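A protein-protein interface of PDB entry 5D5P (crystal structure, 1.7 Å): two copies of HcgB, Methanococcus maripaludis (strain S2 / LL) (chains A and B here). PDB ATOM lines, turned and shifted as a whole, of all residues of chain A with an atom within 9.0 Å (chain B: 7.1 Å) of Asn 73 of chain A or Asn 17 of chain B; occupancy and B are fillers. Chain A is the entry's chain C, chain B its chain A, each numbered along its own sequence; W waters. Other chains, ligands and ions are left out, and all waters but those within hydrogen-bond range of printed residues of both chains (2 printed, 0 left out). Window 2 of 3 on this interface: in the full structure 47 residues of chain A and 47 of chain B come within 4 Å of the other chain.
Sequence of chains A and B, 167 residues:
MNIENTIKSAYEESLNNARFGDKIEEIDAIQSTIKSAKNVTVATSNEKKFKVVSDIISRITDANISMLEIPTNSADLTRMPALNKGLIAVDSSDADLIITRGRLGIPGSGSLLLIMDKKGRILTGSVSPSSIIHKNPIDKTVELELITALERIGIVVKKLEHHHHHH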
ATOM      1  N   ALA A  43      -2.859  17.585  29.531  1.00  0.00           N
ATOM      2  CA  ALA A  43      -3.164  19.000  29.496  1.00  0.00           C
ATOM      3  C   ALA A  43      -3.837  19.369  28.180  1.00  0.00           C
ATOM      4  O   ALA A  43      -3.323  20.174  27.400  1.00  0.00           O
ATOM      5  CB  ALA A  43      -1.870  19.816  29.703  1.00  0.00           C
ATOM      6  N   SER A  45      -8.094  19.464  26.260  1.00  0.00           N
ATOM      7  CA  SER A  45      -9.498  19.117  26.312  1.00  0.00           C
ATOM      8  C   SER A  45      -9.954  18.575  24.960  1.00  0.00           C
ATOM      9  O   SER A  45     -11.170  18.441  24.712  1.00  0.00           O
ATOM     10  CB  SER A  45     -10.359  20.321  26.715  1.00  0.00           C
ATOM     11  OG  SER A  45     -10.144  21.406  25.826  1.00  0.00           O
ATOM     12  N   LEU A  68      -7.618  18.094  31.064  1.00  0.00           N
ATOM     13  CA  LEU A  68      -7.581  19.410  31.699  1.00  0.00           C
ATOM     14  C   LEU A  68      -8.679  20.279  31.054  1.00  0.00           C
ATOM     15  O   LEU A  68      -8.642  20.537  29.852  1.00  0.00           O
ATOM     16  CB  LEU A  68      -6.210  20.043  31.525  1.00  0.00           C
ATOM     17  CG  LEU A  68      -5.923  21.421  32.139  1.00  0.00           C
ATOM     18  CD1 LEU A  68      -5.961  21.421  33.658  1.00  0.00           C
ATOM     19  CD2 LEU A  68      -4.559  21.875  31.647  1.00  0.00           C
ATOM     20  N   GLU A  69      -9.664  20.710  31.813  1.00  0.00           N
ATOM     21  CA  GLU A  69     -10.740  21.457  31.167  1.00  0.00           C
ATOM     22  C   GLU A  69     -10.387  22.945  31.080  1.00  0.00           C
ATOM     23  O   GLU A  69     -10.863  23.652  30.200  1.00  0.00           O
ATOM     24  CB  GLU A  69     -12.086  21.173  31.842  1.00  0.00           C
ATOM     25  CG  GLU A  69     -12.511  19.690  31.647  1.00  0.00           C
ATOM     26  CD  GLU A  69     -12.953  19.350  30.210  1.00  0.00           C
ATOM     27  OE1 GLU A  69     -12.935  20.242  29.331  1.00  0.00           O
ATOM     28  OE2 GLU A  69     -13.299  18.174  29.951  1.00  0.00           O
ATOM     29  N   ILE A  70      -9.544  23.413  31.993  1.00  0.00           N
ATOM     30  CA  ILE A  70      -9.040  24.787  31.933  1.00  0.00           C
ATOM     31  C   ILE A  70      -8.302  25.001  30.596  1.00  0.00           C
ATOM     32  O   ILE A  70      -7.272  24.382  30.360  1.00  0.00           O
ATOM     33  CB  ILE A  70      -8.073  25.053  33.126  1.00  0.00           C
ATOM     34  CG1 ILE A  70      -8.829  24.893  34.448  1.00  0.00           C
ATOM     35  CG2 ILE A  70      -7.425  26.432  33.049  1.00  0.00           C
ATOM     36  CD1 ILE A  70      -7.943  25.089  35.662  1.00  0.00           C
ATOM     37  N   PRO A  71      -8.815  25.894  29.726  1.00  0.00           N
ATOM     38  CA  PRO A  71      -8.085  26.086  28.468  1.00  0.00           C
ATOM     39  C   PRO A  71      -6.673  26.591  28.687  1.00  0.00           C
ATOM     40  O   PRO A  71      -6.350  27.264  29.674  1.00  0.00           O
ATOM     41  CB  PRO A  71      -8.926  27.108  27.697  1.00  0.00           C
ATOM     42  CG  PRO A  71      -9.869  27.685  28.693  1.00  0.00           C
ATOM     43  CD  PRO A  71     -10.092  26.628  29.733  1.00  0.00           C
ATOM     44  N   THR A  72      -5.822  26.241  27.742  1.00  0.00           N
ATOM     45  CA  THR A  72      -4.396  26.407  27.920  1.00  0.00           C
ATOM     46  C   THR A  72      -3.840  27.382  26.888  1.00  0.00           C
ATOM     47  O   THR A  72      -2.625  27.569  26.788  1.00  0.00           O
ATOM     48  CB  THR A  72      -3.680  25.044  27.832  1.00  0.00           C
ATOM     49  OG1 THR A  72      -3.987  24.416  26.576  1.00  0.00           O
ATOM     50  CG2 THR A  72      -4.157  24.145  28.955  1.00  0.00           C
ATOM     51  N   ASN A  73      -4.745  28.006  26.140  1.00  0.00           N
ATOM     52  CA  ASN A  73      -4.366  28.861  25.036  1.00  0.00           C
ATOM     53  C   ASN A  73      -3.484  30.000  25.532  1.00  0.00           C
ATOM     54  O   ASN A  73      -2.592  30.440  24.817  1.00  0.00           O
ATOM     55  CB  ASN A  73      -5.649  29.425  24.361  1.00  0.00           C
ATOM     56  CG  ASN A  73      -5.381  30.064  23.011  1.00  0.00           C
ATOM     57  OD1 ASN A  73      -4.514  29.622  22.256  1.00  0.00           O
ATOM     58  ND2 ASN A  73      -6.128  31.116  22.700  1.00  0.00           N
ATOM     59  N   SER A  74      -3.649  30.367  26.806  1.00  0.00           N
ATOM     60  CA  SER A  74      -2.922  31.499  27.400  1.00  0.00           C
ATOM     61  C   SER A  74      -1.432  31.284  27.413  1.00  0.00           C
ATOM     62  O   SER A  74      -0.635  32.267  27.404  1.00  0.00           O
ATOM     63  CB  SER A  74      -3.406  31.792  28.831  1.00  0.00           C
ATOM     64  OG  SER A  74      -3.106  30.714  29.704  1.00  0.00           O
ATOM     65  N   ALA A  75      -1.050  30.006  27.456  1.00  0.00           N
ATOM     66  CA  ALA A  75       0.351  29.692  27.546  1.00  0.00           C
ATOM     67  C   ALA A  75       1.081  30.052  26.262  1.00  0.00           C
ATOM     68  O   ALA A  75       2.309  30.070  26.266  1.00  0.00           O
ATOM     69  CB  ALA A  75       0.559  28.238  27.887  1.00  0.00           C
ATOM     70  N   ASP A  76       0.356  30.371  25.202  1.00  0.00           N
ATOM     71  CA  ASP A  76       1.040  30.700  23.941  1.00  0.00           C
ATOM     72  C   ASP A  76       1.648  32.094  23.968  1.00  0.00           C
ATOM     73  O   ASP A  76       2.365  32.457  23.047  1.00  0.00           O
ATOM     74  CB  ASP A  76       0.121  30.578  22.726  1.00  0.00           C
ATOM     75  CG  ASP A  76      -0.056  29.138  22.278  1.00  0.00           C
ATOM     76  OD1 ASP A  76       0.638  28.271  22.831  1.00  0.00           O
ATOM     77  OD2 ASP A  76      -0.825  28.892  21.331  1.00  0.00           O
ATOM     78  N   LEU A  77       1.410  32.852  25.034  1.00  0.00           N
ATOM     79  CA  LEU A  77       2.071  34.167  25.184  1.00  0.00           C
ATOM     80  C   LEU A  77       3.160  34.066  26.233  1.00  0.00           C
ATOM     81  O   LEU A  77       3.423  35.011  26.980  1.00  0.00           O
ATOM     82  CB  LEU A  77       1.066  35.265  25.544  1.00  0.00           C
ATOM     83  CG  LEU A  77       0.293  35.766  24.323  1.00  0.00           C
ATOM     84  CD1 LEU A  77      -0.850  34.804  23.981  1.00  0.00           C
ATOM     85  CD2 LEU A  77      -0.230  37.152  24.524  1.00  0.00           C
ATOM     86  N   THR A  78       3.750  32.891  26.349  1.00  0.00           N
ATOM     87  CA  THR A  78       4.856  32.718  27.288  1.00  0.00           C
ATOM     88  C   THR A  78       6.052  32.193  26.522  1.00  0.00           C
ATOM     89  O   THR A  78       5.906  31.688  25.412  1.00  0.00           O
ATOM     90  CB  THR A  78       4.561  31.706  28.441  1.00  0.00           C
ATOM     91  OG1 THR A  78       4.482  30.381  27.895  1.00  0.00           O
ATOM     92  CG2 THR A  78       3.272  32.035  29.172  1.00  0.00           C
ATOM     93  N   PRO A  81       5.618  27.601  25.954  1.00  0.00           N
ATOM     94  CA  PRO A  81       4.192  27.283  26.089  1.00  0.00           C
ATOM     95  C   PRO A  81       3.886  25.879  26.604  1.00  0.00           C
ATOM     96  O   PRO A  81       3.095  25.757  27.534  1.00  0.00           O
ATOM     97  CB  PRO A  81       3.667  27.515  24.667  1.00  0.00           C
ATOM     98  CG  PRO A  81       4.525  28.763  24.227  1.00  0.00           C
ATOM     99  CD  PRO A  81       5.921  28.332  24.696  1.00  0.00           C
ATOM    100  N   ASN A  84       4.483  25.815  30.395  1.00  0.00           N
ATOM    101  CA  ASN A  84       3.527  26.573  31.184  1.00  0.00           C
ATOM    102  C   ASN A  84       2.128  25.980  31.106  1.00  0.00           C
ATOM    103  O   ASN A  84       1.379  26.075  32.070  1.00  0.00           O
ATOM    104  CB  ASN A  84       3.563  28.029  30.742  1.00  0.00           C
ATOM    105  CG  ASN A  84       4.785  28.744  31.291  1.00  0.00           C
ATOM    106  OD1 ASN A  84       5.003  28.771  32.507  1.00  0.00           O
ATOM    107  ND2 ASN A  84       5.615  29.287  30.410  1.00  0.00           N
ATOM    108  N   LYS A  85       1.784  25.297  30.012  1.00  0.00           N
ATOM    109  CA  LYS A  85       0.526  24.546  29.987  1.00  0.00           C
ATOM    110  C   LYS A  85       0.548  23.446  31.033  1.00  0.00           C
ATOM    111  O   LYS A  85      -0.452  23.186  31.715  1.00  0.00           O
ATOM    112  CB  LYS A  85       0.244  23.876  28.633  1.00  0.00           C
ATOM    113  CG  LYS A  85      -0.135  24.693  27.473  1.00  0.00           C
ATOM    114  CD  LYS A  85      -0.655  23.644  26.480  1.00  0.00           C
ATOM    115  CE  LYS A  85      -0.626  24.052  25.058  1.00  0.00           C
ATOM    116  NZ  LYS A  85      -1.160  22.902  24.280  1.00  0.00           N
ATOM    117  N   ILE A  88      -0.099  24.698  34.473  1.00  0.00           N
ATOM    118  CA  ILE A  88      -1.508  24.939  34.797  1.00  0.00           C
ATOM    119  C   ILE A  88      -2.137  23.701  35.472  1.00  0.00           C
ATOM    120  O   ILE A  88      -2.878  23.811  36.452  1.00  0.00           O
ATOM    121  CB  ILE A  88      -2.314  25.306  33.538  1.00  0.00           C
ATOM    122  CG1 ILE A  88      -1.890  26.694  33.033  1.00  0.00           C
ATOM    123  CG2 ILE A  88      -3.822  25.329  33.835  1.00  0.00           C
ATOM    124  CD1 ILE A  88      -2.503  27.085  31.698  1.00  0.00           C
ATOM    125  N   ARG A 103       3.811  24.463  22.110  1.00  0.00           N
ATOM    126  CA  ARG A 103       4.982  25.039  21.458  1.00  0.00           C
ATOM    127  C   ARG A 103       6.235  24.913  22.314  1.00  0.00           C
ATOM    128  O   ARG A 103       6.192  25.025  23.537  1.00  0.00           O
ATOM    129  CB  ARG A 103       4.724  26.506  21.123  1.00  0.00           C
ATOM    130  CG  ARG A 103       5.464  26.972  19.933  1.00  0.00           C
ATOM    131  CD  ARG A 103       4.788  28.197  19.389  1.00  0.00           C
ATOM    132  NE  ARG A 103       4.948  29.301  20.319  1.00  0.00           N
ATOM    133  CZ  ARG A 103       4.012  30.210  20.572  1.00  0.00           C
ATOM    134  NH1 ARG A 103       2.831  30.131  19.990  1.00  0.00           N
ATOM    135  NH2 ARG A 103       4.273  31.188  21.427  1.00  0.00           N
ATOM    136  N   GLU B  12      -0.955  38.575  19.191  1.00  0.00           N
ATOM    137  CA  GLU B  12      -2.220  39.253  18.952  1.00  0.00           C
ATOM    138  C   GLU B  12      -3.297  38.300  18.439  1.00  0.00           C
ATOM    139  O   GLU B  12      -4.477  38.416  18.793  1.00  0.00           O
ATOM    140  CB  GLU B  12      -1.989  40.403  17.981  1.00  0.00           C
ATOM    141  CG  GLU B  12      -1.320  41.598  18.622  1.00  0.00           C
ATOM    142  CD  GLU B  12      -0.649  42.509  17.609  1.00  0.00           C
ATOM    143  OE1 GLU B  12      -0.912  42.365  16.397  1.00  0.00           O
ATOM    144  OE2 GLU B  12       0.138  43.382  18.025  1.00  0.00           O
ATOM    145  N   GLU B  13      -2.894  37.356  17.599  1.00  0.00           N
ATOM    146  CA  GLU B  13      -3.839  36.378  17.073  1.00  0.00           C
ATOM    147  C   GLU B  13      -4.217  35.245  18.054  1.00  0.00           C
ATOM    148  O   GLU B  13      -5.333  34.729  17.960  1.00  0.00           O
ATOM    149  CB  GLU B  13      -3.331  35.826  15.739  1.00  0.00           C
ATOM    150  CG  GLU B  13      -3.098  36.946  14.725  1.00  0.00           C
ATOM    151  CD  GLU B  13      -4.369  37.764  14.456  1.00  0.00           C
ATOM    152  OE1 GLU B  13      -5.353  37.201  13.929  1.00  0.00           O
ATOM    153  OE2 GLU B  13      -4.390  38.975  14.779  1.00  0.00           O
ATOM    154  N   SER B  14      -3.324  34.832  18.967  1.00  0.00           N
ATOM    155  CA  SER B  14      -3.698  33.765  19.919  1.00  0.00           C
ATOM    156  C   SER B  14      -4.843  34.221  20.816  1.00  0.00           C
ATOM    157  O   SER B  14      -5.726  33.436  21.173  1.00  0.00           O
ATOM    158  CB  SER B  14      -2.517  33.338  20.820  1.00  0.00           C
ATOM    159  OG  SER B  14      -1.591  32.469  20.175  1.00  0.00           O
ATOM    160  N   LEU B  15      -4.826  35.508  21.138  1.00  0.00           N
ATOM    161  CA  LEU B  15      -5.818  36.150  21.980  1.00  0.00           C
ATOM    162  C   LEU B  15      -7.150  36.193  21.262  1.00  0.00           C
ATOM    163  O   LEU B  15      -8.223  36.112  21.868  1.00  0.00           O
ATOM    164  CB  LEU B  15      -5.318  37.538  22.353  1.00  0.00           C
ATOM    165  CG  LEU B  15      -4.043  37.438  23.190  1.00  0.00           C
ATOM    166  CD1 LEU B  15      -3.406  38.802  23.281  1.00  0.00           C
ATOM    167  CD2 LEU B  15      -4.282  36.849  24.600  1.00  0.00           C
ATOM    168  N   ASN B  16      -7.054  36.244  19.941  1.00  0.00           N
ATOM    169  CA  ASN B  16      -8.204  36.258  19.062  1.00  0.00           C
ATOM    170  C   ASN B  16      -8.732  34.797  18.966  1.00  0.00           C
ATOM    171  O   ASN B  16      -9.758  34.528  18.317  1.00  0.00           O
ATOM    172  CB  ASN B  16      -7.768  36.936  17.716  1.00  0.00           C
ATOM    173  CG  ASN B  16      -8.640  36.592  16.482  1.00  0.00           C
ATOM    174  OD1 ASN B  16      -9.824  36.269  16.579  1.00  0.00           O
ATOM    175  ND2 ASN B  16      -8.039  36.739  15.297  1.00  0.00           N
ATOM    176  N   ASN B  17      -8.059  33.844  19.639  1.00  0.00           N
ATOM    177  CA  ASN B  17      -8.456  32.432  19.448  1.00  0.00           C
ATOM    178  C   ASN B  17      -8.418  31.992  17.967  1.00  0.00           C
ATOM    179  O   ASN B  17      -9.182  31.126  17.508  1.00  0.00           O
ATOM    180  CB  ASN B  17      -9.865  32.267  20.073  1.00  0.00           C
ATOM    181  CG  ASN B  17      -9.842  32.086  21.574  1.00  0.00           C
ATOM    182  OD1 ASN B  17     -10.267  32.963  22.309  1.00  0.00           O
ATOM    183  ND2 ASN B  17      -9.598  30.818  22.014  1.00  0.00           N
ATOM    184  N   ALA B  18      -7.559  32.699  17.228  1.00  0.00           N
ATOM    185  CA  ALA B  18      -7.317  32.464  15.808  1.00  0.00           C
ATOM    186  C   ALA B  18      -5.959  31.844  15.536  1.00  0.00           C
ATOM    187  O   ALA B  18      -5.478  31.882  14.391  1.00  0.00           O
ATOM    188  CB  ALA B  18      -7.449  33.757  14.991  1.00  0.00           C
ATOM    189  N   ARG B  19      -5.308  31.323  16.569  1.00  0.00           N
ATOM    190  CA  ARG B  19      -4.019  30.711  16.318  1.00  0.00           C
ATOM    191  C   ARG B  19      -4.291  29.284  15.877  1.00  0.00           C
ATOM    192  O   ARG B  19      -4.475  28.386  16.699  1.00  0.00           O
ATOM    193  CB  ARG B  19      -3.122  30.764  17.569  1.00  0.00           C
ATOM    194  CG  ARG B  19      -1.730  30.106  17.403  1.00  0.00           C
ATOM    195  CD  ARG B  19      -0.740  31.048  16.711  1.00  0.00           C
ATOM    196  NE  ARG B  19       0.606  30.488  16.588  1.00  0.00           N
ATOM    197  CZ  ARG B  19       1.481  30.867  15.659  1.00  0.00           C
ATOM    198  NH1 ARG B  19       2.684  30.303  15.612  1.00  0.00           N
ATOM    199  NH2 ARG B  19       1.134  31.777  14.751  1.00  0.00           N
ATOM    200  N   PHE B  20      -4.288  29.081  14.561  1.00  0.00           N
ATOM    201  CA  PHE B  20      -4.648  27.790  13.984  1.00  0.00           C
ATOM    202  C   PHE B  20      -3.530  27.146  13.175  1.00  0.00           C
ATOM    203  O   PHE B  20      -3.772  26.551  12.121  1.00  0.00           O
ATOM    204  CB  PHE B  20      -5.896  27.903  13.107  1.00  0.00           C
ATOM    205  CG  PHE B  20      -7.135  28.305  13.853  1.00  0.00           C
ATOM    206  CD1 PHE B  20      -7.783  27.392  14.669  1.00  0.00           C
ATOM    207  CD2 PHE B  20      -7.716  29.547  13.663  1.00  0.00           C
ATOM    208  CE1 PHE B  20      -8.943  27.732  15.346  1.00  0.00           C
ATOM    209  CE2 PHE B  20      -8.894  29.886  14.329  1.00  0.00           C
ATOM    210  CZ  PHE B  20      -9.504  28.974  15.170  1.00  0.00           C
HETATM  211  O   HOH W   1       1.387  32.690  20.214  1.00  0.00           O
HETATM  212  O   HOH W   2       1.584  27.835  18.461  1.00  0.00           O
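O of Ser 14 of chain B sits at hydrogen-bond distance from ND2 of Asn 73 of chain A (2.8 Å).
The guanidinium group of Arg 103 of chain A is in hydrogen-bond range of the backbone carbonyl oxygen of Asp 76 of chain A (2.8 Å).
Among the printed residues, pairs that only touch across the chains: Asn 73 of chain A with Asn 17 of chain B, Asp 76 of chain A with Ser 14 of chain B, Leu 77 of chain A with Leu 15 of chain B and Leu 77 of chain A with Ser 14 of chain B.
Asn 17 of chain B touches just one residue of chain A: Asn 73 (3.5 Å).
Ser 14 of chain B touches just these residues of chain A: Asn 73, Asp 76 and Leu 77.
No residue of chain A comes within 4 Å of Ala 18 of chain B.
Of the printed residues of chain A, Leu 15 of chain B touches Leu 77 (3.8 Å).
Of the printed residues of chain B, Leu 77 of chain A touches Ser 14 and Leu 15.
Printed residues of chain B within 4 Å of Asp 76 of chain A: Ser 14.
Pro 81 of chain A touches none of the printed residues of chain B.
Asn 84 of chain A touches none of the printed residues of chain B.
The nearest residue of chain B that does not touch Asn 73 of chain A is Leu 15 of chain B (4.8 Å).
The nearest printed residue of chain B that does not touch Asp 76 of chain A is Arg 19 of chain B (4.2 Å).
Hydrophobic or aromatic side chains of chain A within 4 Å of the printed part of chain B: Leu 77.
Hydrophobic or aromatic side chains of chain B within 4 Å of the printed part of chain A: Leu 15.
Among the printed residues, 5 pairs touch across the chains.
No position is printed for both chains.
Water W1 lies within hydrogen-bond range of the guanidinium group of Arg 103 of chain A (2.9 Å), the side-chain hydroxyl of Ser 14 of chain B (3.0 Å) and the backbone carbonyl oxygen of Asp 76 of chain A (3.0 Å).
Water W2 bridges the guanidinium group (NH1) of Arg 103 of chain A and the guanidinium group (NE) of Arg 19 of chain B.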
